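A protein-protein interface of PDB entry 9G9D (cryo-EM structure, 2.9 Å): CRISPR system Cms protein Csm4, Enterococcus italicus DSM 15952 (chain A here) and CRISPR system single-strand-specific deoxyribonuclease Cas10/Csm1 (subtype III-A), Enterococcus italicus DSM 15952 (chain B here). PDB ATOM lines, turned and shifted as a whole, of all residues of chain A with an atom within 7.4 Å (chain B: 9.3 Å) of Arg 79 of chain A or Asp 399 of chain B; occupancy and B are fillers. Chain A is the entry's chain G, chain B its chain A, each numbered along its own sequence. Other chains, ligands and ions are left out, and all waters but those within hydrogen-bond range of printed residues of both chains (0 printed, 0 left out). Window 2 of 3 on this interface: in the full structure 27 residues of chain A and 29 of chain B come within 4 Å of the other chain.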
ATOM      1  N   PRO A  76      -6.810 -12.011 -27.793  1.00  0.00           N
ATOM      2  CA  PRO A  76      -5.508 -11.342 -27.807  1.00  0.00           C
ATOM      3  C   PRO A  76      -4.378 -12.341 -27.988  1.00  0.00           C
ATOM      4  O   PRO A  76      -4.462 -13.496 -27.566  1.00  0.00           O
ATOM      5  CB  PRO A  76      -5.440 -10.666 -26.433  1.00  0.00           C
ATOM      6  CG  PRO A  76      -6.347 -11.478 -25.577  1.00  0.00           C
ATOM      7  CD  PRO A  76      -7.462 -11.927 -26.476  1.00  0.00           C
ATOM      8  N   LEU A  77      -3.311 -11.881 -28.632  1.00  0.00           N
ATOM      9  CA  LEU A  77      -2.129 -12.703 -28.862  1.00  0.00           C
ATOM     10  C   LEU A  77      -1.162 -12.494 -27.703  1.00  0.00           C
ATOM     11  O   LEU A  77      -0.275 -11.638 -27.771  1.00  0.00           O
ATOM     12  CB  LEU A  77      -1.483 -12.355 -30.200  1.00  0.00           C
ATOM     13  CG  LEU A  77      -2.248 -12.825 -31.438  1.00  0.00           C
ATOM     14  CD1 LEU A  77      -1.688 -12.184 -32.693  1.00  0.00           C
ATOM     15  CD2 LEU A  77      -2.199 -14.341 -31.546  1.00  0.00           C
ATOM     16  N   ILE A  78      -1.331 -13.281 -26.643  1.00  0.00           N
ATOM     17  CA  ILE A  78      -0.510 -13.175 -25.445  1.00  0.00           C
ATOM     18  C   ILE A  78       0.012 -14.557 -25.088  1.00  0.00           C
ATOM     19  O   ILE A  78      -0.569 -15.580 -25.463  1.00  0.00           O
ATOM     20  CB  ILE A  78      -1.288 -12.561 -24.260  1.00  0.00           C
ATOM     21  CG1 ILE A  78      -2.605 -13.309 -24.042  1.00  0.00           C
ATOM     22  CG2 ILE A  78      -1.538 -11.081 -24.494  1.00  0.00           C
ATOM     23  CD1 ILE A  78      -3.464 -12.723 -22.945  1.00  0.00           C
ATOM     24  N   ARG A  79       1.123 -14.578 -24.354  1.00  0.00           N
ATOM     25  CA  ARG A  79       1.783 -15.833 -24.025  1.00  0.00           C
ATOM     26  C   ARG A  79       0.932 -16.662 -23.071  1.00  0.00           C
ATOM     27  O   ARG A  79       0.354 -16.141 -22.113  1.00  0.00           O
ATOM     28  CB  ARG A  79       3.153 -15.556 -23.409  1.00  0.00           C
ATOM     29  CG  ARG A  79       4.009 -16.792 -23.201  1.00  0.00           C
ATOM     30  CD  ARG A  79       5.475 -16.428 -23.009  1.00  0.00           C
ATOM     31  NE  ARG A  79       6.058 -15.842 -24.212  1.00  0.00           N
ATOM     32  CZ  ARG A  79       6.218 -14.541 -24.414  1.00  0.00           C
ATOM     33  NH1 ARG A  79       5.858 -13.650 -23.504  1.00  0.00           N
ATOM     34  NH2 ARG A  79       6.753 -14.123 -25.557  1.00  0.00           N
ATOM     35  N   ILE A  80       0.862 -17.963 -23.339  1.00  0.00           N
ATOM     36  CA  ILE A  80       0.107 -18.907 -22.525  1.00  0.00           C
ATOM     37  C   ILE A  80       1.085 -19.903 -21.923  1.00  0.00           C
ATOM     38  O   ILE A  80       1.823 -20.575 -22.654  1.00  0.00           O
ATOM     39  CB  ILE A  80      -0.974 -19.630 -23.346  1.00  0.00           C
ATOM     40  CG1 ILE A  80      -1.887 -18.616 -24.037  1.00  0.00           C
ATOM     41  CG2 ILE A  80      -1.786 -20.555 -22.457  1.00  0.00           C
ATOM     42  CD1 ILE A  80      -2.914 -19.243 -24.954  1.00  0.00           C
ATOM     43  N   GLU A  81       1.088 -20.001 -20.598  1.00  0.00           N
ATOM     44  CA  GLU A  81       2.005 -20.897 -19.902  1.00  0.00           C
ATOM     45  C   GLU A  81       1.441 -22.312 -19.833  1.00  0.00           C
ATOM     46  O   GLU A  81       1.465 -23.050 -20.818  1.00  0.00           O
ATOM     47  CB  GLU A  81       2.301 -20.379 -18.492  1.00  0.00           C
ATOM     48  CG  GLU A  81       1.137 -20.485 -17.516  1.00  0.00           C
ATOM     49  CD  GLU A  81       0.057 -19.447 -17.764  1.00  0.00           C
ATOM     50  OE1 GLU A  81       0.306 -18.496 -18.534  1.00  0.00           O
ATOM     51  OE2 GLU A  81      -1.041 -19.584 -17.187  1.00  0.00           O
ATOM     52  N   TYR A  90      -3.666 -26.346 -25.382  1.00  0.00           N
ATOM     53  CA  TYR A  90      -3.370 -25.340 -26.399  1.00  0.00           C
ATOM     54  C   TYR A  90      -4.319 -25.455 -27.583  1.00  0.00           C
ATOM     55  O   TYR A  90      -4.597 -24.462 -28.264  1.00  0.00           O
ATOM     56  CB  TYR A  90      -1.919 -25.466 -26.859  1.00  0.00           C
ATOM     57  CG  TYR A  90      -0.916 -24.942 -25.858  1.00  0.00           C
ATOM     58  CD1 TYR A  90      -1.312 -24.100 -24.828  1.00  0.00           C
ATOM     59  CD2 TYR A  90       0.425 -25.286 -25.944  1.00  0.00           C
ATOM     60  CE1 TYR A  90      -0.401 -23.616 -23.911  1.00  0.00           C
ATOM     61  CE2 TYR A  90       1.346 -24.807 -25.030  1.00  0.00           C
ATOM     62  CZ  TYR A  90       0.926 -23.973 -24.015  1.00  0.00           C
ATOM     63  OH  TYR A  90       1.837 -23.493 -23.102  1.00  0.00           O
ATOM     64  N   TYR A 107      -9.436 -13.250 -19.457  1.00  0.00           N
ATOM     65  CA  TYR A 107      -8.418 -13.917 -20.310  1.00  0.00           C
ATOM     66  C   TYR A 107      -7.121 -13.124 -20.249  1.00  0.00           C
ATOM     67  O   TYR A 107      -6.036 -13.734 -20.181  1.00  0.00           O
ATOM     68  CB  TYR A 107      -8.946 -13.989 -21.746  1.00  0.00           C
ATOM     69  CG  TYR A 107      -8.106 -14.825 -22.699  1.00  0.00           C
ATOM     70  CD1 TYR A 107      -7.069 -14.260 -23.428  1.00  0.00           C
ATOM     71  CD2 TYR A 107      -8.356 -16.180 -22.871  1.00  0.00           C
ATOM     72  CE1 TYR A 107      -6.301 -15.015 -24.298  1.00  0.00           C
ATOM     73  CE2 TYR A 107      -7.599 -16.946 -23.740  1.00  0.00           C
ATOM     74  CZ  TYR A 107      -6.567 -16.363 -24.453  1.00  0.00           C
ATOM     75  OH  TYR A 107      -5.814 -17.113 -25.308  1.00  0.00           O
ATOM     76  N   GLY A 110      -5.468 -13.796 -17.320  1.00  0.00           N
ATOM     77  CA  GLY A 110      -4.920 -15.133 -17.373  1.00  0.00           C
ATOM     78  C   GLY A 110      -5.645 -16.164 -16.538  1.00  0.00           C
ATOM     79  O   GLY A 110      -5.186 -17.310 -16.464  1.00  0.00           O
ATOM     80  N   ILE A 219      -0.115  -3.678 -21.865  1.00  0.00           N
ATOM     81  CA  ILE A 219      -0.185  -4.202 -23.224  1.00  0.00           C
ATOM     82  C   ILE A 219      -1.321  -3.511 -23.967  1.00  0.00           C
ATOM     83  O   ILE A 219      -2.259  -2.995 -23.350  1.00  0.00           O
ATOM     84  CB  ILE A 219      -0.367  -5.735 -23.227  1.00  0.00           C
ATOM     85  CG1 ILE A 219       0.295  -6.353 -24.457  1.00  0.00           C
ATOM     86  CG2 ILE A 219      -1.840  -6.111 -23.180  1.00  0.00           C
ATOM     87  CD1 ILE A 219       0.355  -7.860 -24.415  1.00  0.00           C
ATOM     88  N   ASP A 239       9.063  -6.286 -29.264  1.00  0.00           N
ATOM     89  CA  ASP A 239       8.278  -6.788 -28.132  1.00  0.00           C
ATOM     90  C   ASP A 239       6.789  -6.854 -28.467  1.00  0.00           C
ATOM     91  O   ASP A 239       5.948  -6.300 -27.758  1.00  0.00           O
ATOM     92  CB  ASP A 239       8.520  -5.941 -26.879  1.00  0.00           C
ATOM     93  CG  ASP A 239       8.002  -6.602 -25.615  1.00  0.00           C
ATOM     94  OD1 ASP A 239       7.590  -7.780 -25.681  1.00  0.00           O
ATOM     95  OD2 ASP A 239       8.006  -5.942 -24.555  1.00  0.00           O
ATOM     96  N   ALA A 240       6.458  -7.536 -29.560  1.00  0.00           N
ATOM     97  CA  ALA A 240       5.083  -7.664 -30.022  1.00  0.00           C
ATOM     98  C   ALA A 240       4.811  -9.098 -30.449  1.00  0.00           C
ATOM     99  O   ALA A 240       5.719  -9.798 -30.908  1.00  0.00           O
ATOM    100  CB  ALA A 240       4.803  -6.708 -31.184  1.00  0.00           C
ATOM    101  N   ARG A 241       3.565  -9.532 -30.289  1.00  0.00           N
ATOM    102  CA  ARG A 241       3.084 -10.795 -30.834  1.00  0.00           C
ATOM    103  C   ARG A 241       1.928 -10.478 -31.772  1.00  0.00           C
ATOM    104  O   ARG A 241       0.885  -9.984 -31.331  1.00  0.00           O
ATOM    105  CB  ARG A 241       2.646 -11.746 -29.721  1.00  0.00           C
ATOM    106  CG  ARG A 241       3.663 -11.891 -28.598  1.00  0.00           C
ATOM    107  CD  ARG A 241       3.144 -12.769 -27.469  1.00  0.00           C
ATOM    108  NE  ARG A 241       3.582 -14.154 -27.594  1.00  0.00           N
ATOM    109  CZ  ARG A 241       2.890 -15.107 -28.203  1.00  0.00           C
ATOM    110  NH1 ARG A 241       1.723 -14.858 -28.771  1.00  0.00           N
ATOM    111  NH2 ARG A 241       3.384 -16.341 -28.244  1.00  0.00           N
ATOM    112  N   THR A 274      -1.062  -8.063 -30.241  1.00  0.00           N
ATOM    113  CA  THR A 274      -0.639  -7.371 -29.033  1.00  0.00           C
ATOM    114  C   THR A 274       0.669  -6.634 -29.277  1.00  0.00           C
ATOM    115  O   THR A 274       1.665  -7.240 -29.684  1.00  0.00           O
ATOM    116  CB  THR A 274      -0.478  -8.351 -27.872  1.00  0.00           C
ATOM    117  OG1 THR A 274       0.374  -9.432 -28.270  1.00  0.00           O
ATOM    118  CG2 THR A 274      -1.830  -8.900 -27.456  1.00  0.00           C
ATOM    119  N   TYR A 276       3.264  -3.808 -27.254  1.00  0.00           N
ATOM    120  CA  TYR A 276       3.545  -3.064 -26.031  1.00  0.00           C
ATOM    121  C   TYR A 276       3.636  -1.569 -26.309  1.00  0.00           C
ATOM    122  O   TYR A 276       3.341  -0.747 -25.434  1.00  0.00           O
ATOM    123  CB  TYR A 276       4.826  -3.582 -25.380  1.00  0.00           C
ATOM    124  CG  TYR A 276       4.589  -4.762 -24.469  1.00  0.00           C
ATOM    125  CD1 TYR A 276       4.274  -4.572 -23.132  1.00  0.00           C
ATOM    126  CD2 TYR A 276       4.663  -6.062 -24.948  1.00  0.00           C
ATOM    127  CE1 TYR A 276       4.048  -5.643 -22.294  1.00  0.00           C
ATOM    128  CE2 TYR A 276       4.440  -7.142 -24.117  1.00  0.00           C
ATOM    129  CZ  TYR A 276       4.132  -6.926 -22.791  1.00  0.00           C
ATOM    130  OH  TYR A 276       3.908  -7.996 -21.958  1.00  0.00           O
ATOM    131  N   ILE A 307      -1.746  -7.902 -18.424  1.00  0.00           N
ATOM    132  CA  ILE A 307      -1.522  -9.341 -18.365  1.00  0.00           C
ATOM    133  C   ILE A 307      -0.670  -9.694 -17.151  1.00  0.00           C
ATOM    134  O   ILE A 307       0.325  -9.030 -16.864  1.00  0.00           O
ATOM    135  CB  ILE A 307      -0.869  -9.864 -19.658  1.00  0.00           C
ATOM    136  CG1 ILE A 307       0.326  -8.994 -20.050  1.00  0.00           C
ATOM    137  CG2 ILE A 307      -1.890  -9.929 -20.782  1.00  0.00           C
ATOM    138  CD1 ILE A 307       1.096  -9.521 -21.238  1.00  0.00           C
ATOM    139  N   GLU B 350      18.956 -20.385 -39.913  1.00  0.00           N
ATOM    140  CA  GLU B 350      17.600 -19.861 -39.786  1.00  0.00           C
ATOM    141  C   GLU B 350      17.421 -18.592 -40.608  1.00  0.00           C
ATOM    142  O   GLU B 350      16.415 -18.435 -41.308  1.00  0.00           O
ATOM    143  CB  GLU B 350      17.267 -19.594 -38.318  1.00  0.00           C
ATOM    144  CG  GLU B 350      15.821 -19.193 -38.082  1.00  0.00           C
ATOM    145  CD  GLU B 350      15.572 -18.708 -36.669  1.00  0.00           C
ATOM    146  OE1 GLU B 350      16.501 -18.132 -36.064  1.00  0.00           O
ATOM    147  OE2 GLU B 350      14.448 -18.906 -36.161  1.00  0.00           O
ATOM    148  N   ALA B 368      10.680 -21.687 -38.300  1.00  0.00           N
ATOM    149  CA  ALA B 368      11.282 -21.099 -37.112  1.00  0.00           C
ATOM    150  C   ALA B 368      12.151 -22.146 -36.433  1.00  0.00           C
ATOM    151  O   ALA B 368      11.798 -23.330 -36.415  1.00  0.00           O
ATOM    152  CB  ALA B 368      10.214 -20.581 -36.146  1.00  0.00           C
ATOM    153  N   ILE B 369      13.283 -21.714 -35.885  1.00  0.00           N
ATOM    154  CA  ILE B 369      14.230 -22.598 -35.213  1.00  0.00           C
ATOM    155  C   ILE B 369      14.509 -22.049 -33.822  1.00  0.00           C
ATOM    156  O   ILE B 369      14.868 -20.875 -33.671  1.00  0.00           O
ATOM    157  CB  ILE B 369      15.530 -22.745 -36.021  1.00  0.00           C
ATOM    158  CG1 ILE B 369      15.264 -23.523 -37.311  1.00  0.00           C
ATOM    159  CG2 ILE B 369      16.605 -23.426 -35.189  1.00  0.00           C
ATOM    160  CD1 ILE B 369      16.511 -23.902 -38.065  1.00  0.00           C
ATOM    161  N   ALA B 370      14.349 -22.898 -32.809  1.00  0.00           N
ATOM    162  CA  ALA B 370      14.637 -22.548 -31.425  1.00  0.00           C
ATOM    163  C   ALA B 370      15.509 -23.631 -30.809  1.00  0.00           C
ATOM    164  O   ALA B 370      15.292 -24.821 -31.057  1.00  0.00           O
ATOM    165  CB  ALA B 370      13.347 -22.377 -30.618  1.00  0.00           C
ATOM    166  N   GLN B 391       9.040 -29.200 -23.812  1.00  0.00           N
ATOM    167  CA  GLN B 391       8.012 -28.184 -23.619  1.00  0.00           C
ATOM    168  C   GLN B 391       8.611 -26.784 -23.629  1.00  0.00           C
ATOM    169  O   GLN B 391       7.977 -25.830 -24.096  1.00  0.00           O
ATOM    170  CB  GLN B 391       7.268 -28.440 -22.308  1.00  0.00           C
ATOM    171  CG  GLN B 391       5.987 -27.639 -22.146  1.00  0.00           C
ATOM    172  CD  GLN B 391       4.858 -28.156 -23.020  1.00  0.00           C
ATOM    173  OE1 GLN B 391       4.988 -29.188 -23.679  1.00  0.00           O
ATOM    174  NE2 GLN B 391       3.740 -27.439 -23.023  1.00  0.00           N
ATOM    175  N   THR B 392       9.844 -26.670 -23.138  1.00  0.00           N
ATOM    176  CA  THR B 392      10.521 -25.360 -23.151  1.00  0.00           C
ATOM    177  C   THR B 392      10.756 -24.961 -24.587  1.00  0.00           C
ATOM    178  O   THR B 392      10.343 -23.842 -24.963  1.00  0.00           O
ATOM    179  CB  THR B 392      11.835 -25.446 -22.378  1.00  0.00           C
ATOM    180  OG1 THR B 392      11.571 -26.279 -21.254  1.00  0.00           O
ATOM    181  CG2 THR B 392      12.319 -24.080 -21.926  1.00  0.00           C
ATOM    182  N   VAL B 393      11.353 -25.854 -25.381  1.00  0.00           N
ATOM    183  CA  VAL B 393      11.704 -25.505 -26.791  1.00  0.00           C
ATOM    184  C   VAL B 393      10.414 -25.201 -27.568  1.00  0.00           C
ATOM    185  O   VAL B 393      10.415 -24.231 -28.352  1.00  0.00           O
ATOM    186  CB  VAL B 393      12.498 -26.641 -27.461  1.00  0.00           C
ATOM    187  CG1 VAL B 393      13.161 -26.178 -28.753  1.00  0.00           C
ATOM    188  CG2 VAL B 393      13.538 -27.222 -26.516  1.00  0.00           C
ATOM    189  N   SER B 394       9.357 -25.985 -27.341  1.00  0.00           N
ATOM    190  CA  SER B 394       8.095 -25.789 -28.099  1.00  0.00           C
ATOM    191  C   SER B 394       7.521 -24.400 -27.792  1.00  0.00           C
ATOM    192  O   SER B 394       7.031 -23.740 -28.728  1.00  0.00           O
ATOM    193  CB  SER B 394       7.095 -26.858 -27.770  1.00  0.00           C
ATOM    194  OG  SER B 394       6.639 -26.719 -26.431  1.00  0.00           O
ATOM    195  N   ARG B 395       7.575 -23.985 -26.526  1.00  0.00           N
ATOM    196  CA  ARG B 395       7.066 -22.641 -26.147  1.00  0.00           C
ATOM    197  C   ARG B 395       7.903 -21.561 -26.853  1.00  0.00           C
ATOM    198  O   ARG B 395       7.300 -20.591 -27.354  1.00  0.00           O
ATOM    199  CB  ARG B 395       7.038 -22.503 -24.621  1.00  0.00           C
ATOM    200  CG  ARG B 395       5.906 -23.354 -24.062  1.00  0.00           C
ATOM    201  CD  ARG B 395       5.830 -23.366 -22.547  1.00  0.00           C
ATOM    202  NE  ARG B 395       4.726 -24.221 -22.097  1.00  0.00           N
ATOM    203  CZ  ARG B 395       4.395 -24.417 -20.829  1.00  0.00           C
ATOM    204  NH1 ARG B 395       3.444 -25.281 -20.521  1.00  0.00           N
ATOM    205  NH2 ARG B 395       5.011 -23.746 -19.873  1.00  0.00           N
ATOM    206  N   LYS B 396       9.225 -21.739 -26.919  1.00  0.00           N
ATOM    207  CA  LYS B 396      10.065 -20.771 -27.668  1.00  0.00           C
ATOM    208  C   LYS B 396       9.660 -20.851 -29.140  1.00  0.00           C
ATOM    209  O   LYS B 396       9.492 -19.792 -29.776  1.00  0.00           O
ATOM    210  CB  LYS B 396      11.556 -21.109 -27.605  1.00  0.00           C
ATOM    211  CG  LYS B 396      12.100 -21.519 -26.253  1.00  0.00           C
ATOM    212  CD  LYS B 396      13.451 -22.211 -26.389  1.00  0.00           C
ATOM    213  CE  LYS B 396      13.919 -22.757 -25.084  1.00  0.00           C
ATOM    214  NZ  LYS B 396      14.061 -21.703 -24.077  1.00  0.00           N
ATOM    215  N   LEU B 397       9.516 -22.076 -29.650  1.00  0.00           N
ATOM    216  CA  LEU B 397       9.128 -22.257 -31.045  1.00  0.00           C
ATOM    217  C   LEU B 397       7.820 -21.537 -31.352  1.00  0.00           C
ATOM    218  O   LEU B 397       7.679 -20.914 -32.410  1.00  0.00           O
ATOM    219  CB  LEU B 397       9.011 -23.748 -31.360  1.00  0.00           C
ATOM    220  CG  LEU B 397       9.100 -24.152 -32.830  1.00  0.00           C
ATOM    221  CD1 LEU B 397      10.432 -23.714 -33.407  1.00  0.00           C
ATOM    222  CD2 LEU B 397       8.915 -25.653 -32.982  1.00  0.00           C
ATOM    223  N   SER B 398       6.849 -21.614 -30.437  1.00  0.00           N
ATOM    224  CA  SER B 398       5.572 -20.941 -30.660  1.00  0.00           C
ATOM    225  C   SER B 398       5.699 -19.434 -30.471  1.00  0.00           C
ATOM    226  O   SER B 398       5.017 -18.659 -31.151  1.00  0.00           O
ATOM    227  CB  SER B 398       4.509 -21.515 -29.724  1.00  0.00           C
ATOM    228  OG  SER B 398       4.284 -22.887 -29.998  1.00  0.00           O
ATOM    229  N   ASP B 399       6.557 -19.001 -29.545  1.00  0.00           N
ATOM    230  CA  ASP B 399       6.801 -17.570 -29.383  1.00  0.00           C
ATOM    231  C   ASP B 399       7.442 -16.978 -30.630  1.00  0.00           C
ATOM    232  O   ASP B 399       7.134 -15.847 -31.021  1.00  0.00           O
ATOM    233  CB  ASP B 399       7.679 -17.317 -28.159  1.00  0.00           C
ATOM    234  CG  ASP B 399       6.914 -17.435 -26.859  1.00  0.00           C
ATOM    235  OD1 ASP B 399       5.709 -17.759 -26.906  1.00  0.00           O
ATOM    236  OD2 ASP B 399       7.515 -17.201 -25.790  1.00  0.00           O
ATOM    237  N   LYS B 400       8.350 -17.724 -31.260  1.00  0.00           N
ATOM    238  CA  LYS B 400       8.980 -17.239 -32.482  1.00  0.00           C
ATOM    239  C   LYS B 400       7.978 -17.185 -33.630  1.00  0.00           C
ATOM    240  O   LYS B 400       8.046 -16.291 -34.480  1.00  0.00           O
ATOM    241  CB  LYS B 400      10.174 -18.120 -32.839  1.00  0.00           C
ATOM    242  CG  LYS B 400      11.255 -17.408 -33.630  1.00  0.00           C
ATOM    243  CD  LYS B 400      12.546 -18.204 -33.615  1.00  0.00           C
ATOM    244  CE  LYS B 400      13.010 -18.454 -32.191  1.00  0.00           C
ATOM    245  NZ  LYS B 400      14.251 -19.271 -32.143  1.00  0.00           N
ATOM    246  N   LYS B 401       7.041 -18.136 -33.670  1.00  0.00           N
ATOM    247  CA  LYS B 401       5.981 -18.081 -34.672  1.00  0.00           C
ATOM    248  C   LYS B 401       5.068 -16.883 -34.446  1.00  0.00           C
ATOM    249  O   LYS B 401       4.411 -16.409 -35.379  1.00  0.00           O
ATOM    250  CB  LYS B 401       5.174 -19.381 -34.667  1.00  0.00           C
ATOM    251  CG  LYS B 401       5.831 -20.525 -35.421  1.00  0.00           C
ATOM    252  CD  LYS B 401       4.827 -21.619 -35.759  1.00  0.00           C
ATOM    253  CE  LYS B 401       4.420 -22.413 -34.530  1.00  0.00           C
ATOM    254  NZ  LYS B 401       5.542 -23.244 -34.013  1.00  0.00           N
ATOM    255  N   ALA B 402       5.005 -16.386 -33.209  1.00  0.00           N
ATOM    256  CA  ALA B 402       4.212 -15.191 -32.935  1.00  0.00           C
ATOM    257  C   ALA B 402       4.811 -13.971 -33.619  1.00  0.00           C
ATOM    258  O   ALA B 402       4.091 -13.166 -34.218  1.00  0.00           O
ATOM    259  CB  ALA B 402       4.097 -14.966 -31.429  1.00  0.00           C
ATOM    260  N   HIS B 403       6.132 -13.811 -33.540  1.00  0.00           N
ATOM    261  CA  HIS B 403       6.768 -12.696 -34.233  1.00  0.00           C
ATOM    262  C   HIS B 403       6.954 -13.017 -35.712  1.00  0.00           C
ATOM    263  O   HIS B 403       6.356 -12.369 -36.580  1.00  0.00           O
ATOM    264  CB  HIS B 403       8.108 -12.378 -33.572  1.00  0.00           C
ATOM    265  CG  HIS B 403       8.488 -10.933 -33.637  1.00  0.00           C
ATOM    266  ND1 HIS B 403       9.295 -10.419 -34.629  1.00  0.00           N
ATOM    267  CD2 HIS B 403       8.179  -9.894 -32.827  1.00  0.00           C
ATOM    268  CE1 HIS B 403       9.464  -9.125 -34.427  1.00  0.00           C
ATOM    269  NE2 HIS B 403       8.796  -8.781 -33.342  1.00  0.00           N
ATOM    270  N   LYS B 404       7.789 -14.010 -36.015  1.00  0.00           N
ATOM    271  CA  LYS B 404       7.882 -14.696 -37.303  1.00  0.00           C
ATOM    272  C   LYS B 404       8.447 -13.822 -38.419  1.00  0.00           C
ATOM    273  O   LYS B 404       8.764 -14.342 -39.496  1.00  0.00           O
ATOM    274  CB  LYS B 404       6.523 -15.268 -37.732  1.00  0.00           C
ATOM    275  CG  LYS B 404       6.594 -16.337 -38.816  1.00  0.00           C
ATOM    276  CD  LYS B 404       5.227 -16.928 -39.122  1.00  0.00           C
ATOM    277  CE  LYS B 404       4.922 -18.117 -38.226  1.00  0.00           C
ATOM    278  NZ  LYS B 404       3.610 -18.739 -38.563  1.00  0.00           N
ATOM    279  N   TYR B 405       8.631 -12.524 -38.185  1.00  0.00           N
ATOM    280  CA  TYR B 405       9.120 -11.619 -39.218  1.00  0.00           C
ATOM    281  C   TYR B 405       9.774 -10.418 -38.551  1.00  0.00           C
ATOM    282  O   TYR B 405       9.504 -10.102 -37.391  1.00  0.00           O
ATOM    283  CB  TYR B 405       7.997 -11.180 -40.166  1.00  0.00           C
ATOM    284  CG  TYR B 405       7.550 -12.275 -41.106  1.00  0.00           C
ATOM    285  CD1 TYR B 405       8.377 -12.713 -42.131  1.00  0.00           C
ATOM    286  CD2 TYR B 405       6.312 -12.882 -40.959  1.00  0.00           C
ATOM    287  CE1 TYR B 405       7.982 -13.721 -42.986  1.00  0.00           C
ATOM    288  CE2 TYR B 405       5.906 -13.891 -41.811  1.00  0.00           C
ATOM    289  CZ  TYR B 405       6.745 -14.306 -42.822  1.00  0.00           C
ATOM    290  OH  TYR B 405       6.347 -15.310 -43.673  1.00  0.00           O
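OD2 of Asp 399 of chain B is in salt-bridge range of NE of Arg 79 of chain A, 2.5 Å away.
The guanidinium group of Arg 241 of chain A lies within salt-bridge range of the side-chain carboxylate of Asp 399 of chain B (3.0 Å).
NE of Arg 395 of chain B lies within hydrogen-bond range of OH of Tyr 90 of chain A (3.1 Å).
The guanidinium group of Arg 395 of chain B is in hydrogen-bond range of the backbone carbonyl oxygen of Glu 81 of chain A (3.0 Å).
Printed residues of chain B within 4 Å of Arg 79 of chain A: Asp 399 (2.5 Å).
Asp 399 of chain B touches just these residues of chain A: Arg 79 and Arg 241.
No residue of chain B comes within 4 Å of Ile 80 of chain A.
Of the printed residues of chain A, His 403 of chain B touches Ala 240 (3.1 Å).
Of the printed residues of chain B, Tyr 90 of chain A touches Arg 395 (3.1 Å).
The nearest residue of chain A that does not touch Asp 399 of chain B is Ile 80 of chain A (6.0 Å).
N of Thr 274 of chain A sits at hydrogen-bond distance from O of Arg 241 of chain A.
A ring nitrogen (ND1) of His 403 of chain B lies within hydrogen-bond range of the backbone carbonyl oxygen (O) of Tyr 405 of chain B (2.8 Å).
The side-chain amide nitrogen (NE2) of Gln 391 of chain B lies close to the guanidinium group (NH1) of Arg 395 of chain B, 3.3 Å away.
O of Ile 80 of chain A is in hydrogen-bond range of OH of Tyr 90 of chain A.
Among the printed residues, pairs that only touch across the chains: Ala 240 of chain A with His 403 of chain B (3.1 Å) and Arg 241 of chain A with Ala 402 of chain B (3.4 Å).
Among the printed residues, 6 pairs touch across the chains.
Among the printed residues, Asp or Glu carboxylates within 4 Å of a Lys or Arg side-chain nitrogen of the other chain: Arg 79 of chain A with Asp 399 of chain B and Arg 241 of chain A with Asp 399 of chain B.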
